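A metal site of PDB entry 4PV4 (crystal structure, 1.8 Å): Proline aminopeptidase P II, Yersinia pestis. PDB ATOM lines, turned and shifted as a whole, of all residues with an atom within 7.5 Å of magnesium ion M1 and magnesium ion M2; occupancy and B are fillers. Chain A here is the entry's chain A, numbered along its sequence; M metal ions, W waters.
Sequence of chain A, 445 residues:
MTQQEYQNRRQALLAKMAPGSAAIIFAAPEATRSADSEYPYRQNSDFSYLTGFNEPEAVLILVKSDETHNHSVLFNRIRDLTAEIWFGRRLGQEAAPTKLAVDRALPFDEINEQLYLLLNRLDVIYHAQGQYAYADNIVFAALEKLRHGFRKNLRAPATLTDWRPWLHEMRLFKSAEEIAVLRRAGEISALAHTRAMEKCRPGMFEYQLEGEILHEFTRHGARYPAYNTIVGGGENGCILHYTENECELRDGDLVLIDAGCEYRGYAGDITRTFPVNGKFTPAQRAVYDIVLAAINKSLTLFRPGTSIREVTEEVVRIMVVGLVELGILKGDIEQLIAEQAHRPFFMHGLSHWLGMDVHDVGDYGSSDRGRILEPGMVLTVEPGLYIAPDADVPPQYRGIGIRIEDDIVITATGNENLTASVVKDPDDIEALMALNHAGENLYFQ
CG2 of Thr 380 touches magnesium ion M1 (3.7 Å).
Five residues have an atom within 4 Å of magnesium ion M1: Asp 269, His 352, Thr 380, Glu 382 and Glu 405.
OG1 of Thr 271 is in hydrogen-bond range of NE of Arg 403 (3.2 Å).
The side-chain hydroxyl (OG1) of Thr 380 sits close to the side-chain carboxylate (OE2) of Glu 382 (2.8 Å).
The backbone NH (N) of Gly 260 lies within hydrogen-bond range of the side-chain hydroxyl (OH) of Tyr 227, 3.1 Å away.
O of Thr 380 lies within hydrogen-bond range of OG of Ser 351 (2.7 Å).
The backbone NH (N) of Glu 382 is in hydrogen-bond range of the backbone carbonyl oxygen (O) of Leu 350 (2.8 Å).
N of Glu 405 is in hydrogen-bond range of O of Thr 271, at 3.0 Å.
O of Ile 230 lies within hydrogen-bond range of N of Asp 258 (2.9 Å).
A ring nitrogen (ND1) of His 352 lies close to the backbone carbonyl oxygen (O) of Val 358 (2.9 Å).
Magnesium ion M1 is bound by water W1, 2.0 Å away.
Magnesium ion M1 is bound by OE2 of Glu 405, at 2.1 Å.
Magnesium ion M1 is bound by a ring nitrogen (NE2) of His 352.
OD2 of Asp 269 is bound to magnesium ion M1, 2.3 Å away.
The side-chain carboxylate (OE2) of Glu 382 binds magnesium ion M1.
OH of Tyr 227 touches magnesium ion M2, 3.9 Å away.
OG1 of Thr 271 touches magnesium ion M2, at 3.5 Å.
OD1 of Asp 269 binds magnesium ion M2, at 2.1 Å.
Magnesium ion M2 is bound by OE1 of Glu 405, at 2.2 Å.
Magnesium ion M2 is bound by water W1 (2.2 Å).
OD1 of Asp 258 is bound to magnesium ion M2 (2.3 Å).
Magnesium ion M2 is bound by the side-chain carboxylate (OD2) of Asp 258.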
ATOM      1  N   TYR A 227      31.613  20.446  20.836  1.00  0.00           N
ATOM      2  CA  TYR A 227      31.274  20.320  22.255  1.00  0.00           C
ATOM      3  C   TYR A 227      30.224  19.224  22.403  1.00  0.00           C
ATOM      4  O   TYR A 227      29.663  18.783  21.381  1.00  0.00           O
ATOM      5  CB  TYR A 227      30.721  21.641  22.796  1.00  0.00           C
ATOM      6  CG  TYR A 227      29.545  22.191  22.041  1.00  0.00           C
ATOM      7  CD1 TYR A 227      29.733  22.992  20.928  1.00  0.00           C
ATOM      8  CD2 TYR A 227      28.246  21.885  22.410  1.00  0.00           C
ATOM      9  CE1 TYR A 227      28.673  23.462  20.192  1.00  0.00           C
ATOM     10  CE2 TYR A 227      27.151  22.383  21.682  1.00  0.00           C
ATOM     11  CZ  TYR A 227      27.387  23.172  20.582  1.00  0.00           C
ATOM     12  OH  TYR A 227      26.361  23.667  19.818  1.00  0.00           O
ATOM     13  N   ILE A 230      23.734  18.693  23.505  1.00  0.00           N
ATOM     14  CA  ILE A 230      22.641  18.712  24.514  1.00  0.00           C
ATOM     15  C   ILE A 230      21.383  18.326  23.746  1.00  0.00           C
ATOM     16  O   ILE A 230      21.094  19.006  22.739  1.00  0.00           O
ATOM     17  CB  ILE A 230      22.459  20.121  25.013  1.00  0.00           C
ATOM     18  CG1 ILE A 230      23.680  20.486  25.851  1.00  0.00           C
ATOM     19  CG2 ILE A 230      21.129  20.299  25.797  1.00  0.00           C
ATOM     20  CD1 ILE A 230      23.901  21.972  25.890  1.00  0.00           C
ATOM     21  N   ILE A 257      17.814  21.251  21.584  1.00  0.00           N
ATOM     22  CA  ILE A 257      19.011  20.681  21.058  1.00  0.00           C
ATOM     23  C   ILE A 257      20.062  21.750  20.814  1.00  0.00           C
ATOM     24  O   ILE A 257      19.866  22.694  19.977  1.00  0.00           O
ATOM     25  CB  ILE A 257      18.731  19.958  19.714  1.00  0.00           C
ATOM     26  CG1 ILE A 257      17.684  18.873  19.925  1.00  0.00           C
ATOM     27  CG2 ILE A 257      20.043  19.395  19.185  1.00  0.00           C
ATOM     28  CD1 ILE A 257      17.464  18.000  18.693  1.00  0.00           C
ATOM     29  N   ASP A 258      21.196  21.588  21.457  1.00  0.00           N
ATOM     30  CA  ASP A 258      22.301  22.497  21.276  1.00  0.00           C
ATOM     31  C   ASP A 258      23.464  21.675  20.756  1.00  0.00           C
ATOM     32  O   ASP A 258      23.937  20.729  21.450  1.00  0.00           O
ATOM     33  CB  ASP A 258      22.605  23.185  22.605  1.00  0.00           C
ATOM     34  CG  ASP A 258      23.699  24.250  22.493  1.00  0.00           C
ATOM     35  OD1 ASP A 258      24.377  24.407  21.426  1.00  0.00           O
ATOM     36  OD2 ASP A 258      23.790  25.087  23.451  1.00  0.00           O
ATOM     37  N   ALA A 259      23.842  21.921  19.486  1.00  0.00           N
ATOM     38  CA  ALA A 259      24.843  21.087  18.838  1.00  0.00           C
ATOM     39  C   ALA A 259      25.546  21.873  17.764  1.00  0.00           C
ATOM     40  O   ALA A 259      24.956  22.769  17.149  1.00  0.00           O
ATOM     41  CB  ALA A 259      24.225  19.848  18.221  1.00  0.00           C
ATOM     42  N   GLY A 260      26.809  21.540  17.544  1.00  0.00           N
ATOM     43  CA  GLY A 260      27.600  22.272  16.555  1.00  0.00           C
ATOM     44  C   GLY A 260      28.843  21.460  16.186  1.00  0.00           C
ATOM     45  O   GLY A 260      29.431  20.778  17.059  1.00  0.00           O
ATOM     46  N   GLY A 268      30.854  25.479  14.882  1.00  0.00           N
ATOM     47  CA  GLY A 268      29.489  25.978  14.847  1.00  0.00           C
ATOM     48  C   GLY A 268      28.864  25.783  16.230  1.00  0.00           C
ATOM     49  O   GLY A 268      29.340  24.954  17.034  1.00  0.00           O
ATOM     50  N   ASP A 269      27.759  26.463  16.462  1.00  0.00           N
ATOM     51  CA  ASP A 269      27.052  26.351  17.715  1.00  0.00           C
ATOM     52  C   ASP A 269      25.652  26.816  17.530  1.00  0.00           C
ATOM     53  O   ASP A 269      25.407  28.041  17.447  1.00  0.00           O
ATOM     54  CB  ASP A 269      27.731  27.237  18.706  1.00  0.00           C
ATOM     55  CG  ASP A 269      27.217  27.121  20.100  1.00  0.00           C
ATOM     56  OD1 ASP A 269      26.237  26.422  20.374  1.00  0.00           O
ATOM     57  OD2 ASP A 269      27.803  27.912  20.912  1.00  0.00           O
ATOM     58  N   ILE A 270      24.736  25.872  17.341  1.00  0.00           N
ATOM     59  CA  ILE A 270      23.321  26.206  17.075  1.00  0.00           C
ATOM     60  C   ILE A 270      22.505  25.605  18.198  1.00  0.00           C
ATOM     61  O   ILE A 270      22.747  24.474  18.629  1.00  0.00           O
ATOM     62  CB  ILE A 270      22.860  25.633  15.740  1.00  0.00           C
ATOM     63  CG1 ILE A 270      23.637  26.300  14.628  1.00  0.00           C
ATOM     64  CG2 ILE A 270      21.355  25.780  15.553  1.00  0.00           C
ATOM     65  CD1 ILE A 270      23.376  25.701  13.259  1.00  0.00           C
ATOM     66  N   THR A 271      21.462  26.349  18.608  1.00  0.00           N
ATOM     67  CA  THR A 271      20.425  25.748  19.446  1.00  0.00           C
ATOM     68  C   THR A 271      19.111  25.944  18.724  1.00  0.00           C
ATOM     69  O   THR A 271      18.787  27.034  18.225  1.00  0.00           O
ATOM     70  CB  THR A 271      20.335  26.350  20.872  1.00  0.00           C
ATOM     71  OG1 THR A 271      21.632  26.273  21.516  1.00  0.00           O
ATOM     72  CG2 THR A 271      19.319  25.589  21.655  1.00  0.00           C
ATOM     73  N   GLY A 349      24.530  34.400  29.644  1.00  0.00           N
ATOM     74  CA  GLY A 349      24.786  35.477  28.697  1.00  0.00           C
ATOM     75  C   GLY A 349      24.018  35.333  27.399  1.00  0.00           C
ATOM     76  O   GLY A 349      23.695  34.209  26.965  1.00  0.00           O
ATOM     77  N   LEU A 350      23.785  36.460  26.734  1.00  0.00           N
ATOM     78  CA  LEU A 350      23.193  36.450  25.405  1.00  0.00           C
ATOM     79  C   LEU A 350      24.106  35.945  24.316  1.00  0.00           C
ATOM     80  O   LEU A 350      23.658  35.399  23.259  1.00  0.00           O
ATOM     81  CB  LEU A 350      22.790  37.879  25.030  1.00  0.00           C
ATOM     82  CG  LEU A 350      22.070  38.024  23.701  1.00  0.00           C
ATOM     83  CD1 LEU A 350      20.715  37.344  23.601  1.00  0.00           C
ATOM     84  CD2 LEU A 350      21.822  39.490  23.431  1.00  0.00           C
ATOM     85  N   SER A 351      25.399  36.155  24.513  1.00  0.00           N
ATOM     86  CA  SER A 351      26.361  35.941  23.445  1.00  0.00           C
ATOM     87  C   SER A 351      27.724  35.600  23.985  1.00  0.00           C
ATOM     88  O   SER A 351      28.143  36.150  25.039  1.00  0.00           O
ATOM     89  CB  SER A 351      26.566  37.242  22.643  1.00  0.00           C
ATOM     90  OG  SER A 351      25.390  37.674  22.013  1.00  0.00           O
ATOM     91  N   HIS A 352      28.416  34.708  23.282  1.00  0.00           N
ATOM     92  CA  HIS A 352      29.874  34.508  23.498  1.00  0.00           C
ATOM     93  C   HIS A 352      30.595  34.506  22.136  1.00  0.00           C
ATOM     94  O   HIS A 352      30.033  34.201  21.109  1.00  0.00           O
ATOM     95  CB  HIS A 352      30.175  33.205  24.286  1.00  0.00           C
ATOM     96  CG  HIS A 352      29.627  31.985  23.639  1.00  0.00           C
ATOM     97  ND1 HIS A 352      30.259  31.334  22.600  1.00  0.00           N
ATOM     98  CD2 HIS A 352      28.490  31.286  23.897  1.00  0.00           C
ATOM     99  CE1 HIS A 352      29.519  30.303  22.223  1.00  0.00           C
ATOM    100  NE2 HIS A 352      28.483  30.218  23.034  1.00  0.00           N
ATOM    101  N   TRP A 353      31.858  34.870  22.150  1.00  0.00           N
ATOM    102  CA  TRP A 353      32.685  34.789  20.992  1.00  0.00           C
ATOM    103  C   TRP A 353      32.700  33.365  20.492  1.00  0.00           C
ATOM    104  O   TRP A 353      32.606  32.413  21.315  1.00  0.00           O
ATOM    105  CB  TRP A 353      34.154  35.175  21.360  1.00  0.00           C
ATOM    106  CG  TRP A 353      34.355  36.472  22.022  1.00  0.00           C
ATOM    107  CD1 TRP A 353      35.107  36.674  23.149  1.00  0.00           C
ATOM    108  CD2 TRP A 353      33.849  37.774  21.641  1.00  0.00           C
ATOM    109  NE1 TRP A 353      35.110  37.992  23.489  1.00  0.00           N
ATOM    110  CE2 TRP A 353      34.315  38.679  22.624  1.00  0.00           C
ATOM    111  CE3 TRP A 353      33.017  38.239  20.643  1.00  0.00           C
ATOM    112  CZ2 TRP A 353      34.045  40.020  22.570  1.00  0.00           C
ATOM    113  CZ3 TRP A 353      32.710  39.622  20.603  1.00  0.00           C
ATOM    114  CH2 TRP A 353      33.231  40.476  21.582  1.00  0.00           C
ATOM    115  N   LEU A 354      32.931  33.192  19.204  1.00  0.00           N
ATOM    116  CA  LEU A 354      32.949  31.883  18.537  1.00  0.00           C
ATOM    117  C   LEU A 354      34.154  31.819  17.586  1.00  0.00           C
ATOM    118  O   LEU A 354      34.509  32.802  16.944  1.00  0.00           O
ATOM    119  CB  LEU A 354      31.641  31.679  17.760  1.00  0.00           C
ATOM    120  CG  LEU A 354      31.493  30.363  17.056  1.00  0.00           C
ATOM    121  CD1 LEU A 354      31.260  29.311  18.095  1.00  0.00           C
ATOM    122  CD2 LEU A 354      30.275  30.434  16.177  1.00  0.00           C
ATOM    123  N   VAL A 358      34.467  26.838  20.956  1.00  0.00           N
ATOM    124  CA  VAL A 358      33.092  27.258  21.092  1.00  0.00           C
ATOM    125  C   VAL A 358      32.881  28.419  22.011  1.00  0.00           C
ATOM    126  O   VAL A 358      32.191  29.408  21.584  1.00  0.00           O
ATOM    127  CB  VAL A 358      32.152  26.065  21.346  1.00  0.00           C
ATOM    128  CG1 VAL A 358      32.407  25.416  22.689  1.00  0.00           C
ATOM    129  CG2 VAL A 358      30.676  26.513  21.184  1.00  0.00           C
ATOM    130  N   HIS A 359      33.519  28.455  23.178  1.00  0.00           N
ATOM    131  CA  HIS A 359      33.539  29.627  23.977  1.00  0.00           C
ATOM    132  C   HIS A 359      34.847  30.335  23.627  1.00  0.00           C
ATOM    133  O   HIS A 359      35.896  30.057  24.230  1.00  0.00           O
ATOM    134  CB  HIS A 359      33.431  29.318  25.479  1.00  0.00           C
ATOM    135  CG  HIS A 359      32.081  28.815  25.898  1.00  0.00           C
ATOM    136  ND1 HIS A 359      31.872  28.094  27.051  1.00  0.00           N
ATOM    137  CD2 HIS A 359      30.907  28.851  25.255  1.00  0.00           C
ATOM    138  CE1 HIS A 359      30.600  27.715  27.101  1.00  0.00           C
ATOM    139  NE2 HIS A 359      29.991  28.174  26.033  1.00  0.00           N
ATOM    140  N   LEU A 379      30.309  35.727  16.924  1.00  0.00           N
ATOM    141  CA  LEU A 379      29.642  35.538  18.188  1.00  0.00           C
ATOM    142  C   LEU A 379      28.326  34.825  18.037  1.00  0.00           C
ATOM    143  O   LEU A 379      27.725  34.762  16.962  1.00  0.00           O
ATOM    144  CB  LEU A 379      29.441  36.844  18.944  1.00  0.00           C
ATOM    145  CG  LEU A 379      28.620  37.947  18.279  1.00  0.00           C
ATOM    146  CD1 LEU A 379      27.965  38.890  19.288  1.00  0.00           C
ATOM    147  CD2 LEU A 379      29.432  38.713  17.261  1.00  0.00           C
ATOM    148  N   THR A 380      27.902  34.200  19.131  1.00  0.00           N
ATOM    149  CA  THR A 380      26.623  33.555  19.177  1.00  0.00           C
ATOM    150  C   THR A 380      25.551  34.574  19.594  1.00  0.00           C
ATOM    151  O   THR A 380      25.814  35.604  20.266  1.00  0.00           O
ATOM    152  CB  THR A 380      26.612  32.363  20.131  1.00  0.00           C
ATOM    153  OG1 THR A 380      26.781  32.784  21.507  1.00  0.00           O
ATOM    154  CG2 THR A 380      27.709  31.344  19.759  1.00  0.00           C
ATOM    155  N   VAL A 381      24.313  34.242  19.308  1.00  0.00           N
ATOM    156  CA  VAL A 381      23.178  35.004  19.800  1.00  0.00           C
ATOM    157  C   VAL A 381      22.156  33.976  20.315  1.00  0.00           C
ATOM    158  O   VAL A 381      21.626  33.202  19.507  1.00  0.00           O
ATOM    159  CB  VAL A 381      22.512  35.840  18.691  1.00  0.00           C
ATOM    160  CG1 VAL A 381      21.316  36.646  19.216  1.00  0.00           C
ATOM    161  CG2 VAL A 381      23.562  36.698  17.952  1.00  0.00           C
ATOM    162  N   GLU A 382      21.990  33.892  21.627  1.00  0.00           N
ATOM    163  CA  GLU A 382      21.389  32.754  22.266  1.00  0.00           C
ATOM    164  C   GLU A 382      20.497  33.061  23.454  1.00  0.00           C
ATOM    165  O   GLU A 382      20.621  32.514  24.517  1.00  0.00           O
ATOM    166  CB  GLU A 382      22.464  31.720  22.586  1.00  0.00           C
ATOM    167  CG  GLU A 382      23.531  32.180  23.550  1.00  0.00           C
ATOM    168  CD  GLU A 382      24.464  31.011  23.775  1.00  0.00           C
ATOM    169  OE1 GLU A 382      23.921  29.969  24.190  1.00  0.00           O
ATOM    170  OE2 GLU A 382      25.644  31.100  23.457  1.00  0.00           O
ATOM    171  N   ARG A 403      15.698  27.590  24.114  1.00  0.00           N
ATOM    172  CA  ARG A 403      16.749  28.450  23.704  1.00  0.00           C
ATOM    173  C   ARG A 403      16.763  28.412  22.181  1.00  0.00           C
ATOM    174  O   ARG A 403      16.532  27.379  21.549  1.00  0.00           O
ATOM    175  CB  ARG A 403      18.091  27.989  24.346  1.00  0.00           C
ATOM    176  CG  ARG A 403      19.282  28.772  23.800  1.00  0.00           C
ATOM    177  CD  ARG A 403      20.628  28.636  24.455  1.00  0.00           C
ATOM    178  NE  ARG A 403      21.169  27.267  24.474  1.00  0.00           N
ATOM    179  CZ  ARG A 403      21.048  26.380  25.438  1.00  0.00           C
ATOM    180  NH1 ARG A 403      21.664  25.225  25.309  1.00  0.00           N
ATOM    181  NH2 ARG A 403      20.363  26.599  26.540  1.00  0.00           N
ATOM    182  N   GLU A 405      19.451  29.803  19.130  1.00  0.00           N
ATOM    183  CA  GLU A 405      20.839  30.311  19.015  1.00  0.00           C
ATOM    184  C   GLU A 405      21.348  30.226  17.611  1.00  0.00           C
ATOM    185  O   GLU A 405      21.303  29.109  16.998  1.00  0.00           O
ATOM    186  CB  GLU A 405      21.760  29.481  19.885  1.00  0.00           C
ATOM    187  CG  GLU A 405      23.223  29.823  19.715  1.00  0.00           C
ATOM    188  CD  GLU A 405      24.109  29.059  20.668  1.00  0.00           C
ATOM    189  OE1 GLU A 405      23.682  28.030  21.208  1.00  0.00           O
ATOM    190  OE2 GLU A 405      25.238  29.537  20.951  1.00  0.00           O
ATOM    191  N   ASP A 406      21.795  31.347  17.086  1.00  0.00           N
ATOM    192  CA  ASP A 406      22.460  31.422  15.776  1.00  0.00           C
ATOM    193  C   ASP A 406      23.891  31.945  16.013  1.00  0.00           C
ATOM    194  O   ASP A 406      24.186  32.515  17.110  1.00  0.00           O
ATOM    195  CB  ASP A 406      21.751  32.399  14.841  1.00  0.00           C
ATOM    196  CG  ASP A 406      20.540  31.791  14.184  1.00  0.00           C
ATOM    197  OD1 ASP A 406      20.506  30.550  13.991  1.00  0.00           O
ATOM    198  OD2 ASP A 406      19.626  32.607  13.859  1.00  0.00           O
ATOM    199  N   ASP A 407      24.713  31.816  14.994  1.00  0.00           N
ATOM    200  CA  ASP A 407      26.128  32.280  14.972  1.00  0.00           C
ATOM    201  C   ASP A 407      26.192  33.407  13.923  1.00  0.00           C
ATOM    202  O   ASP A 407      25.725  33.215  12.752  1.00  0.00           O
ATOM    203  CB  ASP A 407      27.054  31.179  14.555  1.00  0.00           C
ATOM    204  CG  ASP A 407      26.921  29.956  15.420  1.00  0.00           C
ATOM    205  OD1 ASP A 407      26.542  30.122  16.595  1.00  0.00           O
ATOM    206  OD2 ASP A 407      27.164  28.829  14.880  1.00  0.00           O
HETATM  207 MG    MG M   1      26.628  29.122  22.458  1.00  0.00          MG
HETATM  208 MG    MG M   2      25.064  26.525  22.109  1.00  0.00          MG
HETATM  209  O   HOH W   1      25.594  27.942  23.764  1.00  0.00           O
